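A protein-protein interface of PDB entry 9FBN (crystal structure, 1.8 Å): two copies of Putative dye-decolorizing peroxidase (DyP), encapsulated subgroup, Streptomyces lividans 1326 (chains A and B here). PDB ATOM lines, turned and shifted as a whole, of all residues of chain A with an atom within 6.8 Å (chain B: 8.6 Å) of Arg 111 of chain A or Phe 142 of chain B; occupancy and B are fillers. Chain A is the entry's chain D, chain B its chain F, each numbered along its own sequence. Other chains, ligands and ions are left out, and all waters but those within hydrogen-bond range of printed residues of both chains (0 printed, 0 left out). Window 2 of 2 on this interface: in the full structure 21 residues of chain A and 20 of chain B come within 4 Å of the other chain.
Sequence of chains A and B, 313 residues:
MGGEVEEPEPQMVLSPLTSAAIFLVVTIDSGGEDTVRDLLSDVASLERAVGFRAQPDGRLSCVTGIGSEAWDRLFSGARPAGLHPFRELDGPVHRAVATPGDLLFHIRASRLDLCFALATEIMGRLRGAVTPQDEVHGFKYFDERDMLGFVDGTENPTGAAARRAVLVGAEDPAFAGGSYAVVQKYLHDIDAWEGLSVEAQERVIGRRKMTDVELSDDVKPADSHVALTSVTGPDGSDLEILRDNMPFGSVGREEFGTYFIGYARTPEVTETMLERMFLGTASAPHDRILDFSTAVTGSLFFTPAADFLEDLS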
ATOM      1  N   SER A  19      15.154  26.578   2.430  1.00  0.00           N
ATOM      2  CA  SER A  19      14.970  26.873   1.031  1.00  0.00           C
ATOM      3  C   SER A  19      14.824  25.615   0.156  1.00  0.00           C
ATOM      4  O   SER A  19      14.403  25.760  -0.982  1.00  0.00           O
ATOM      5  CB  SER A  19      16.143  27.705   0.492  1.00  0.00           C
ATOM      6  OG  SER A  19      17.382  27.089   0.778  1.00  0.00           O
ATOM      7  N   ALA A  20      15.222  24.433   0.646  1.00  0.00           N
ATOM      8  CA  ALA A  20      14.983  23.228  -0.132  1.00  0.00           C
ATOM      9  C   ALA A  20      14.378  22.122   0.722  1.00  0.00           C
ATOM     10  O   ALA A  20      14.645  22.001   1.925  1.00  0.00           O
ATOM     11  CB  ALA A  20      16.267  22.732  -0.826  1.00  0.00           C
ATOM     12  N   ALA A  21      13.712  21.225  -0.008  1.00  0.00           N
ATOM     13  CA  ALA A  21      13.070  20.056   0.572  1.00  0.00           C
ATOM     14  C   ALA A  21      12.929  18.913  -0.436  1.00  0.00           C
ATOM     15  O   ALA A  21      12.773  19.098  -1.659  1.00  0.00           O
ATOM     16  CB  ALA A  21      11.776  20.425   1.241  1.00  0.00           C
ATOM     17  N   VAL A  50      24.945  12.577   7.650  1.00  0.00           N
ATOM     18  CA  VAL A  50      24.926  13.368   6.458  1.00  0.00           C
ATOM     19  C   VAL A  50      25.169  14.848   6.788  1.00  0.00           C
ATOM     20  O   VAL A  50      25.857  15.520   6.002  1.00  0.00           O
ATOM     21  CB  VAL A  50      23.643  13.155   5.619  1.00  0.00           C
ATOM     22  CG1 VAL A  50      23.532  14.077   4.390  1.00  0.00           C
ATOM     23  CG2 VAL A  50      23.548  11.698   5.159  1.00  0.00           C
ATOM     24  N   ARG A  53      28.850  17.346   8.853  1.00  0.00           N
ATOM     25  CA  ARG A  53      30.018  17.929   8.219  1.00  0.00           C
ATOM     26  C   ARG A  53      29.699  19.178   7.396  1.00  0.00           C
ATOM     27  O   ARG A  53      30.631  19.947   7.078  1.00  0.00           O
ATOM     28  CB  ARG A  53      30.768  16.997   7.278  1.00  0.00           C
ATOM     29  CG  ARG A  53      30.088  16.339   6.105  1.00  0.00           C
ATOM     30  CD  ARG A  53      31.105  15.376   5.533  1.00  0.00           C
ATOM     31  NE  ARG A  53      30.573  14.806   4.299  1.00  0.00           N
ATOM     32  CZ  ARG A  53      29.609  13.912   4.253  1.00  0.00           C
ATOM     33  NH1 ARG A  53      29.077  13.469   5.354  1.00  0.00           N
ATOM     34  NH2 ARG A  53      29.185  13.465   3.085  1.00  0.00           N
ATOM     35  N   ALA A  54      28.386  19.369   7.110  1.00  0.00           N
ATOM     36  CA  ALA A  54      27.890  20.521   6.366  1.00  0.00           C
ATOM     37  C   ALA A  54      27.378  21.649   7.276  1.00  0.00           C
ATOM     38  O   ALA A  54      26.829  22.634   6.767  1.00  0.00           O
ATOM     39  CB  ALA A  54      26.805  20.039   5.413  1.00  0.00           C
ATOM     40  N   GLN A  55      27.528  21.518   8.609  1.00  0.00           N
ATOM     41  CA  GLN A  55      27.000  22.495   9.555  1.00  0.00           C
ATOM     42  C   GLN A  55      27.942  23.702   9.670  1.00  0.00           C
ATOM     43  O   GLN A  55      29.108  23.599   9.275  1.00  0.00           O
ATOM     44  CB  GLN A  55      26.904  21.898  10.968  1.00  0.00           C
ATOM     45  CG  GLN A  55      25.700  21.000  11.213  1.00  0.00           C
ATOM     46  CD  GLN A  55      25.605  20.508  12.639  1.00  0.00           C
ATOM     47  OE1 GLN A  55      25.298  19.335  12.894  1.00  0.00           O
ATOM     48  NE2 GLN A  55      25.850  21.407  13.577  1.00  0.00           N
ATOM     49  N   ASP A  57      25.573  25.757   8.322  1.00  0.00           N
ATOM     50  CA  ASP A  57      24.742  26.339   7.270  1.00  0.00           C
ATOM     51  C   ASP A  57      23.730  25.358   6.654  1.00  0.00           C
ATOM     52  O   ASP A  57      22.768  25.795   6.015  1.00  0.00           O
ATOM     53  CB  ASP A  57      25.578  26.910   6.132  1.00  0.00           C
ATOM     54  CG  ASP A  57      26.391  28.154   6.472  1.00  0.00           C
ATOM     55  OD1 ASP A  57      26.128  28.730   7.559  1.00  0.00           O
ATOM     56  OD2 ASP A  57      27.263  28.538   5.643  1.00  0.00           O
ATOM     57  N   GLY A  58      23.950  24.051   6.821  1.00  0.00           N
ATOM     58  CA  GLY A  58      23.196  23.022   6.103  1.00  0.00           C
ATOM     59  C   GLY A  58      21.712  22.968   6.491  1.00  0.00           C
ATOM     60  O   GLY A  58      20.862  22.919   5.582  1.00  0.00           O
ATOM     61  N   LEU A  60      20.121  20.608   7.866  1.00  0.00           N
ATOM     62  CA  LEU A  60      19.491  19.340   7.452  1.00  0.00           C
ATOM     63  C   LEU A  60      18.674  18.762   8.589  1.00  0.00           C
ATOM     64  O   LEU A  60      19.181  18.574   9.722  1.00  0.00           O
ATOM     65  CB  LEU A  60      20.567  18.332   7.046  1.00  0.00           C
ATOM     66  CG  LEU A  60      20.039  16.946   6.579  1.00  0.00           C
ATOM     67  CD1 LEU A  60      19.209  17.117   5.335  1.00  0.00           C
ATOM     68  CD2 LEU A  60      21.218  16.050   6.178  1.00  0.00           C
ATOM     69  N   ARG A 108      14.421  18.397   4.955  1.00  0.00           N
ATOM     70  CA  ARG A 108      14.618  19.814   4.668  1.00  0.00           C
ATOM     71  C   ARG A 108      16.101  20.186   4.890  1.00  0.00           C
ATOM     72  O   ARG A 108      16.720  19.643   5.808  1.00  0.00           O
ATOM     73  CB  ARG A 108      13.717  20.607   5.611  1.00  0.00           C
ATOM     74  CG  ARG A 108      12.242  20.680   5.222  1.00  0.00           C
ATOM     75  CD  ARG A 108      11.421  21.449   6.258  1.00  0.00           C
ATOM     76  NE  ARG A 108      11.221  20.711   7.486  1.00  0.00           N
ATOM     77  CZ  ARG A 108      10.287  20.934   8.426  1.00  0.00           C
ATOM     78  NH1 ARG A 108       9.450  21.943   8.231  1.00  0.00           N
ATOM     79  NH2 ARG A 108      10.216  20.176   9.519  1.00  0.00           N
ATOM     80  N   ALA A 109      16.559  21.228   4.157  1.00  0.00           N
ATOM     81  CA  ALA A 109      17.912  21.783   4.277  1.00  0.00           C
ATOM     82  C   ALA A 109      17.989  23.121   3.550  1.00  0.00           C
ATOM     83  O   ALA A 109      17.040  23.562   2.900  1.00  0.00           O
ATOM     84  CB  ALA A 109      18.952  20.812   3.733  1.00  0.00           C
ATOM     85  N   SER A 110      19.175  23.770   3.625  1.00  0.00           N
ATOM     86  CA  SER A 110      19.431  25.004   2.939  1.00  0.00           C
ATOM     87  C   SER A 110      19.851  24.785   1.493  1.00  0.00           C
ATOM     88  O   SER A 110      19.778  25.726   0.670  1.00  0.00           O
ATOM     89  CB  SER A 110      20.382  25.904   3.752  1.00  0.00           C
ATOM     90  OG  SER A 110      21.672  25.332   3.921  1.00  0.00           O
ATOM     91  N   ARG A 111      20.159  23.537   1.128  1.00  0.00           N
ATOM     92  CA  ARG A 111      20.519  23.203  -0.250  1.00  0.00           C
ATOM     93  C   ARG A 111      20.029  21.802  -0.646  1.00  0.00           C
ATOM     94  O   ARG A 111      20.137  20.913   0.167  1.00  0.00           O
ATOM     95  CB  ARG A 111      22.039  22.948  -0.401  1.00  0.00           C
ATOM     96  CG  ARG A 111      23.079  23.694   0.408  1.00  0.00           C
ATOM     97  CD  ARG A 111      24.459  23.102   0.142  1.00  0.00           C
ATOM     98  NE  ARG A 111      24.775  22.925  -1.282  1.00  0.00           N
ATOM     99  CZ  ARG A 111      25.688  23.586  -1.966  1.00  0.00           C
ATOM    100  NH1 ARG A 111      26.232  24.741  -1.549  1.00  0.00           N
ATOM    101  NH2 ARG A 111      26.031  23.093  -3.129  1.00  0.00           N
ATOM    102  N   LEU A 112      19.666  21.618  -1.900  1.00  0.00           N
ATOM    103  CA  LEU A 112      19.058  20.367  -2.368  1.00  0.00           C
ATOM    104  C   LEU A 112      19.992  19.157  -2.285  1.00  0.00           C
ATOM    105  O   LEU A 112      19.481  18.050  -2.171  1.00  0.00           O
ATOM    106  CB  LEU A 112      18.515  20.516  -3.774  1.00  0.00           C
ATOM    107  CG  LEU A 112      17.533  19.451  -4.279  1.00  0.00           C
ATOM    108  CD1 LEU A 112      16.408  19.219  -3.258  1.00  0.00           C
ATOM    109  CD2 LEU A 112      16.919  19.856  -5.616  1.00  0.00           C
ATOM    110  N   ASP A 113      21.332  19.367  -2.349  1.00  0.00           N
ATOM    111  CA  ASP A 113      22.260  18.255  -2.394  1.00  0.00           C
ATOM    112  C   ASP A 113      22.277  17.479  -1.063  1.00  0.00           C
ATOM    113  O   ASP A 113      22.287  16.238  -1.103  1.00  0.00           O
ATOM    114  CB  ASP A 113      23.570  18.779  -2.947  1.00  0.00           C
ATOM    115  CG  ASP A 113      23.999  20.071  -2.272  1.00  0.00           C
ATOM    116  OD1 ASP A 113      23.380  21.135  -2.610  1.00  0.00           O
ATOM    117  OD2 ASP A 113      24.914  19.972  -1.431  1.00  0.00           O
ATOM    118  N   LEU A 114      22.157  18.155   0.064  1.00  0.00           N
ATOM    119  CA  LEU A 114      22.051  17.562   1.379  1.00  0.00           C
ATOM    120  C   LEU A 114      20.754  16.764   1.504  1.00  0.00           C
ATOM    121  O   LEU A 114      20.803  15.732   2.181  1.00  0.00           O
ATOM    122  CB  LEU A 114      22.107  18.518   2.569  1.00  0.00           C
ATOM    123  CG  LEU A 114      23.433  19.265   2.823  1.00  0.00           C
ATOM    124  CD1 LEU A 114      23.167  20.381   3.824  1.00  0.00           C
ATOM    125  CD2 LEU A 114      24.569  18.317   3.298  1.00  0.00           C
ATOM    126  N   CYS A 115      19.612  17.332   1.022  1.00  0.00           N
ATOM    127  CA  CYS A 115      18.355  16.564   1.038  1.00  0.00           C
ATOM    128  C   CYS A 115      18.540  15.265   0.253  1.00  0.00           C
ATOM    129  O   CYS A 115      18.112  14.197   0.736  1.00  0.00           O
ATOM    130  CB  CYS A 115      17.211  17.371   0.418  1.00  0.00           C
ATOM    131  SG  CYS A 115      16.828  18.813   1.452  1.00  0.00           S
ATOM    132  N   PHE A 116      19.104  15.375  -0.990  1.00  0.00           N
ATOM    133  CA  PHE A 116      19.277  14.243  -1.905  1.00  0.00           C
ATOM    134  C   PHE A 116      20.194  13.170  -1.281  1.00  0.00           C
ATOM    135  O   PHE A 116      19.919  11.946  -1.355  1.00  0.00           O
ATOM    136  CB  PHE A 116      19.829  14.685  -3.264  1.00  0.00           C
ATOM    137  CG  PHE A 116      19.678  13.624  -4.349  1.00  0.00           C
ATOM    138  CD1 PHE A 116      18.537  13.567  -5.143  1.00  0.00           C
ATOM    139  CD2 PHE A 116      20.674  12.703  -4.576  1.00  0.00           C
ATOM    140  CE1 PHE A 116      18.373  12.548  -6.056  1.00  0.00           C
ATOM    141  CE2 PHE A 116      20.539  11.758  -5.547  1.00  0.00           C
ATOM    142  CZ  PHE A 116      19.403  11.672  -6.291  1.00  0.00           C
ATOM    143  N   THR B  18      28.568  28.149  -9.522  1.00  0.00           N
ATOM    144  CA  THR B  18      27.141  28.125  -9.203  1.00  0.00           C
ATOM    145  C   THR B  18      26.753  26.743  -8.736  1.00  0.00           C
ATOM    146  O   THR B  18      27.304  25.757  -9.189  1.00  0.00           O
ATOM    147  CB  THR B  18      26.290  28.577 -10.403  1.00  0.00           C
ATOM    148  OG1 THR B  18      26.910  28.099 -11.598  1.00  0.00           O
ATOM    149  CG2 THR B  18      26.322  30.072 -10.579  1.00  0.00           C
ATOM    150  N   SER B  19      25.765  26.698  -7.823  1.00  0.00           N
ATOM    151  CA  SER B  19      25.334  25.497  -7.149  1.00  0.00           C
ATOM    152  C   SER B  19      24.030  24.953  -7.742  1.00  0.00           C
ATOM    153  O   SER B  19      23.610  23.868  -7.414  1.00  0.00           O
ATOM    154  CB  SER B  19      25.159  25.779  -5.695  1.00  0.00           C
ATOM    155  OG  SER B  19      24.193  26.832  -5.572  1.00  0.00           O
ATOM    156  N   ALA B  20      23.437  25.617  -8.753  1.00  0.00           N
ATOM    157  CA  ALA B  20      22.229  25.109  -9.355  1.00  0.00           C
ATOM    158  C   ALA B  20      22.202  25.487 -10.819  1.00  0.00           C
ATOM    159  O   ALA B  20      22.693  26.516 -11.238  1.00  0.00           O
ATOM    160  CB  ALA B  20      20.956  25.620  -8.629  1.00  0.00           C
ATOM    161  N   ARG B  59      23.526  35.532  -8.839  1.00  0.00           N
ATOM    162  CA  ARG B  59      24.438  35.044  -9.892  1.00  0.00           C
ATOM    163  C   ARG B  59      23.726  34.350 -11.074  1.00  0.00           C
ATOM    164  O   ARG B  59      24.326  33.480 -11.717  1.00  0.00           O
ATOM    165  CB  ARG B  59      25.469  34.051  -9.312  1.00  0.00           C
ATOM    166  CG  ARG B  59      26.242  34.596  -8.126  1.00  0.00           C
ATOM    167  CD  ARG B  59      27.186  33.611  -7.443  1.00  0.00           C
ATOM    168  NE  ARG B  59      27.225  34.092  -6.053  1.00  0.00           N
ATOM    169  CZ  ARG B  59      27.178  33.350  -4.948  1.00  0.00           C
ATOM    170  NH1 ARG B  59      27.770  32.172  -4.901  1.00  0.00           N
ATOM    171  NH2 ARG B  59      26.667  33.859  -3.842  1.00  0.00           N
ATOM    172  N   SER B 110      22.850  30.814  -8.070  1.00  0.00           N
ATOM    173  CA  SER B 110      23.184  30.332  -6.740  1.00  0.00           C
ATOM    174  C   SER B 110      22.025  29.555  -6.130  1.00  0.00           C
ATOM    175  O   SER B 110      22.233  28.858  -5.120  1.00  0.00           O
ATOM    176  CB  SER B 110      23.623  31.443  -5.831  1.00  0.00           C
ATOM    177  OG  SER B 110      22.600  32.427  -5.715  1.00  0.00           O
ATOM    178  N   ARG B 111      20.818  29.630  -6.745  1.00  0.00           N
ATOM    179  CA  ARG B 111      19.654  28.882  -6.262  1.00  0.00           C
ATOM    180  C   ARG B 111      18.674  28.507  -7.382  1.00  0.00           C
ATOM    181  O   ARG B 111      18.604  29.188  -8.401  1.00  0.00           O
ATOM    182  CB  ARG B 111      18.766  29.719  -5.333  1.00  0.00           C
ATOM    183  CG  ARG B 111      19.348  30.937  -4.645  1.00  0.00           C
ATOM    184  CD  ARG B 111      18.325  31.689  -3.803  1.00  0.00           C
ATOM    185  NE  ARG B 111      17.119  31.010  -3.328  1.00  0.00           N
ATOM    186  CZ  ARG B 111      16.643  31.072  -2.096  1.00  0.00           C
ATOM    187  NH1 ARG B 111      17.338  31.666  -1.153  1.00  0.00           N
ATOM    188  NH2 ARG B 111      15.447  30.602  -1.803  1.00  0.00           N
ATOM    189  N   LEU B 112      17.916  27.433  -7.181  1.00  0.00           N
ATOM    190  CA  LEU B 112      17.182  26.742  -8.232  1.00  0.00           C
ATOM    191  C   LEU B 112      15.919  27.505  -8.657  1.00  0.00           C
ATOM    192  O   LEU B 112      15.572  27.557  -9.834  1.00  0.00           O
ATOM    193  CB  LEU B 112      16.844  25.345  -7.763  1.00  0.00           C
ATOM    194  CG  LEU B 112      16.208  24.433  -8.810  1.00  0.00           C
ATOM    195  CD1 LEU B 112      17.103  24.216 -10.065  1.00  0.00           C
ATOM    196  CD2 LEU B 112      15.943  23.116  -8.148  1.00  0.00           C
ATOM    197  N   GLY B 138      19.855  20.570 -12.106  1.00  0.00           N
ATOM    198  CA  GLY B 138      21.080  20.071 -11.451  1.00  0.00           C
ATOM    199  C   GLY B 138      21.420  20.792 -10.162  1.00  0.00           C
ATOM    200  O   GLY B 138      20.948  21.894  -9.904  1.00  0.00           O
ATOM    201  N   PHE B 139      22.251  20.134  -9.310  1.00  0.00           N
ATOM    202  CA  PHE B 139      22.610  20.607  -8.011  1.00  0.00           C
ATOM    203  C   PHE B 139      24.037  20.097  -7.697  1.00  0.00           C
ATOM    204  O   PHE B 139      24.346  18.944  -7.872  1.00  0.00           O
ATOM    205  CB  PHE B 139      21.675  20.175  -6.888  1.00  0.00           C
ATOM    206  CG  PHE B 139      21.373  18.694  -6.871  1.00  0.00           C
ATOM    207  CD1 PHE B 139      22.138  17.831  -6.088  1.00  0.00           C
ATOM    208  CD2 PHE B 139      20.304  18.194  -7.590  1.00  0.00           C
ATOM    209  CE1 PHE B 139      21.853  16.465  -6.104  1.00  0.00           C
ATOM    210  CE2 PHE B 139      20.015  16.841  -7.568  1.00  0.00           C
ATOM    211  CZ  PHE B 139      20.807  15.989  -6.820  1.00  0.00           C
ATOM    212  N   LYS B 140      24.901  21.009  -7.318  1.00  0.00           N
ATOM    213  CA  LYS B 140      26.272  20.655  -6.968  1.00  0.00           C
ATOM    214  C   LYS B 140      26.276  20.234  -5.510  1.00  0.00           C
ATOM    215  O   LYS B 140      25.396  20.623  -4.732  1.00  0.00           O
ATOM    216  CB  LYS B 140      27.107  21.861  -7.389  1.00  0.00           C
ATOM    217  CG  LYS B 140      28.548  21.672  -7.807  1.00  0.00           C
ATOM    218  CD  LYS B 140      28.718  20.734  -8.990  1.00  0.00           C
ATOM    219  CE  LYS B 140      28.761  19.400  -8.375  1.00  0.00           C
ATOM    220  NZ  LYS B 140      29.198  19.444  -6.989  1.00  0.00           N
ATOM    221  N   TYR B 141      27.108  19.247  -5.180  1.00  0.00           N
ATOM    222  CA  TYR B 141      27.391  18.853  -3.812  1.00  0.00           C
ATOM    223  C   TYR B 141      28.280  19.924  -3.171  1.00  0.00           C
ATOM    224  O   TYR B 141      28.970  20.742  -3.843  1.00  0.00           O
ATOM    225  CB  TYR B 141      28.052  17.487  -3.581  1.00  0.00           C
ATOM    226  CG  TYR B 141      27.097  16.311  -3.841  1.00  0.00           C
ATOM    227  CD1 TYR B 141      26.157  15.896  -2.909  1.00  0.00           C
ATOM    228  CD2 TYR B 141      27.077  15.704  -5.068  1.00  0.00           C
ATOM    229  CE1 TYR B 141      25.254  14.874  -3.187  1.00  0.00           C
ATOM    230  CE2 TYR B 141      26.215  14.662  -5.370  1.00  0.00           C
ATOM    231  CZ  TYR B 141      25.276  14.260  -4.436  1.00  0.00           C
ATOM    232  OH  TYR B 141      24.440  13.245  -4.824  1.00  0.00           O
ATOM    233  N   PHE B 142      28.266  19.901  -1.834  1.00  0.00           N
ATOM    234  CA  PHE B 142      28.737  21.087  -1.127  1.00  0.00           C
ATOM    235  C   PHE B 142      30.269  21.191  -1.183  1.00  0.00           C
ATOM    236  O   PHE B 142      30.823  22.284  -0.943  1.00  0.00           O
ATOM    237  CB  PHE B 142      28.160  21.067   0.286  1.00  0.00           C
ATOM    238  CG  PHE B 142      29.023  20.253   1.231  1.00  0.00           C
ATOM    239  CD1 PHE B 142      28.760  18.913   1.465  1.00  0.00           C
ATOM    240  CD2 PHE B 142      30.025  20.860   1.953  1.00  0.00           C
ATOM    241  CE1 PHE B 142      29.560  18.171   2.322  1.00  0.00           C
ATOM    242  CE2 PHE B 142      30.800  20.128   2.859  1.00  0.00           C
ATOM    243  CZ  PHE B 142      30.590  18.782   3.002  1.00  0.00           C
ATOM    244  N   ASP B 143      30.954  20.063  -1.469  1.00  0.00           N
ATOM    245  CA  ASP B 143      32.414  20.096  -1.692  1.00  0.00           C
ATOM    246  C   ASP B 143      32.816  19.857  -3.138  1.00  0.00           C
ATOM    247  O   ASP B 143      33.847  19.253  -3.427  1.00  0.00           O
ATOM    248  CB  ASP B 143      33.160  19.112  -0.813  1.00  0.00           C
ATOM    249  CG  ASP B 143      32.562  17.711  -0.736  1.00  0.00           C
ATOM    250  OD1 ASP B 143      31.510  17.430  -1.432  1.00  0.00           O
ATOM    251  OD2 ASP B 143      33.169  16.934  -0.026  1.00  0.00           O
ATOM    252  N   GLU B 144      31.950  20.259  -4.066  1.00  0.00           N
ATOM    253  CA  GLU B 144      32.255  20.222  -5.468  1.00  0.00           C
ATOM    254  C   GLU B 144      32.345  18.800  -6.009  1.00  0.00           C
ATOM    255  O   GLU B 144      32.944  18.630  -7.066  1.00  0.00           O
ATOM    256  CB  GLU B 144      33.474  21.046  -5.904  1.00  0.00           C
ATOM    257  CG  GLU B 144      33.226  22.519  -5.611  1.00  0.00           C
ATOM    258  CD  GLU B 144      32.053  23.161  -6.349  1.00  0.00           C
ATOM    259  OE1 GLU B 144      31.792  22.822  -7.483  1.00  0.00           O
ATOM    260  OE2 GLU B 144      31.460  24.100  -5.827  1.00  0.00           O
ATOM    261  N   ARG B 145      31.793  17.832  -5.299  1.00  0.00           N
ATOM    262  CA  ARG B 145      31.789  16.441  -5.696  1.00  0.00           C
ATOM    263  C   ARG B 145      30.672  16.090  -6.673  1.00  0.00           C
ATOM    264  O   ARG B 145      29.644  16.752  -6.709  1.00  0.00           O
ATOM    265  CB  ARG B 145      31.774  15.562  -4.452  1.00  0.00           C
ATOM    266  CG  ARG B 145      33.128  15.553  -3.758  1.00  0.00           C
ATOM    267  CD  ARG B 145      33.125  14.695  -2.513  1.00  0.00           C
ATOM    268  NE  ARG B 145      34.337  14.999  -1.787  1.00  0.00           N
ATOM    269  CZ  ARG B 145      35.552  14.476  -1.958  1.00  0.00           C
ATOM    270  NH1 ARG B 145      35.802  13.510  -2.851  1.00  0.00           N
ATOM    271  NH2 ARG B 145      36.541  14.963  -1.248  1.00  0.00           N
ATOM    272  N   ASP B 146      30.894  15.034  -7.502  1.00  0.00           N
ATOM    273  CA  ASP B 146      29.874  14.563  -8.434  1.00  0.00           C
ATOM    274  C   ASP B 146      29.259  13.308  -7.813  1.00  0.00           C
ATOM    275  O   ASP B 146      29.651  12.869  -6.739  1.00  0.00           O
ATOM    276  CB  ASP B 146      30.468  14.393  -9.815  1.00  0.00           C
ATOM    277  CG  ASP B 146      31.557  13.319  -9.906  1.00  0.00           C
ATOM    278  OD1 ASP B 146      31.702  12.456  -9.006  1.00  0.00           O
ATOM    279  OD2 ASP B 146      32.338  13.416 -10.885  1.00  0.00           O
ATOM    280  N   MET B 246      27.126  18.721 -13.769  1.00  0.00           N
ATOM    281  CA  MET B 246      26.162  18.915 -12.667  1.00  0.00           C
ATOM    282  C   MET B 246      25.506  17.573 -12.375  1.00  0.00           C
ATOM    283  O   MET B 246      25.024  16.925 -13.276  1.00  0.00           O
ATOM    284  CB  MET B 246      25.066  19.938 -13.055  1.00  0.00           C
ATOM    285  CG  MET B 246      25.576  21.354 -13.120  1.00  0.00           C
ATOM    286  SD  MET B 246      26.149  22.057 -11.559  1.00  0.00           S
ATOM    287  CE  MET B 246      24.747  22.308 -10.471  1.00  0.00           C
ATOM    288  N   PRO B 247      25.522  17.115 -11.120  1.00  0.00           N
ATOM    289  CA  PRO B 247      24.702  16.007 -10.680  1.00  0.00           C
ATOM    290  C   PRO B 247      23.217  16.297 -10.833  1.00  0.00           C
ATOM    291  O   PRO B 247      22.848  17.443 -10.846  1.00  0.00           O
ATOM    292  CB  PRO B 247      25.053  15.762  -9.216  1.00  0.00           C
ATOM    293  CG  PRO B 247      26.346  16.573  -8.961  1.00  0.00           C
ATOM    294  CD  PRO B 247      26.349  17.630 -10.040  1.00  0.00           C
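Ser 19 of chain A touches Arg 111 of chain B, and with the chains exchanged Arg 111 of chain A touches Ser 19 of chain B. 5 positions are printed for both chains. Of the 12 pairs that touch across the chains among the printed residues, 2 have their exchanged pair printed and touching as well.
The guanidinium group (NE) of Arg 111 of chain A is in salt-bridge range of the side-chain carboxylate (OD1) of Asp 113 of chain A (2.6 Å). O of Ser 110 of chain A sits at hydrogen-bond distance from OG of Ser 19 of chain A (2.8 Å). The backbone carbonyl oxygen (O) of Ser 19 of chain B lies within hydrogen-bond range of the backbone NH (N) of Lys 140 of chain B (3.1 Å). The backbone NH of Phe 139 of chain B lies within hydrogen-bond range of the backbone carbonyl oxygen of Pro 247 of chain B, at 3.2 Å. The backbone carbonyl oxygen of Ser 110 of chain B is in hydrogen-bond range of the side-chain hydroxyl of Ser 19 of chain B (2.9 Å). O of Arg 145 of chain B sits at hydrogen-bond distance from NZ of Lys 140 of chain B (2.7 Å).
Among the printed residues, merely in contact across the chains: Asp 113 of chain A with Phe 139 of chain B, Phe 116 of chain A with Phe 139 of chain B, Asp 113 of chain A with Tyr 141 of chain B, Ser 19 of chain A with Arg 111 of chain B, Phe 116 of chain A with Tyr 141 of chain B, Arg 111 of chain A with Ser 19 of chain B, Arg 111 of chain A with Tyr 141 of chain B, Arg 111 of chain A with Phe 142 of chain B and Arg 53 of chain A with Phe 142 of chain B.
Of the 19 printed residues of chain A, 5 touch a printed residue of chain B. Among the printed residues, 12 pairs touch across the chains. Among the printed residues, no Asp or Glu carboxylate lies within 4 Å of a Lys or Arg side-chain nitrogen of the other chain.
O of Lys 140 of chain B sits close to OD1 of Asp 113 of chain A (3.0 Å). NH2 of Arg 111 of chain A is in hydrogen-bond range of O of Lys 140 of chain B (3.0 Å). The side-chain carboxylate of Asp 113 of chain A lies within hydrogen-bond range of the backbone NH of Phe 142 of chain B, at 3.4 Å.
Of the printed residues of chain B, Asp 113 of chain A touches Phe 139 (3.6 Å), Lys 140 (2.9 Å), Tyr 141 (3.6 Å) and Phe 142 (3.4 Å). Of the printed residues of chain A, Ser 19 of chain B touches Arg 111. Printed residues of chain A within 4 Å of Lys 140 of chain B: Arg 111 and Asp 113. Of the printed residues of chain A, Tyr 141 of chain B touches Arg 111, Asp 113 and Phe 116. The nearest printed residue of chain A that does not touch Phe 142 of chain B is Ala 54 of chain A (4.5 Å).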
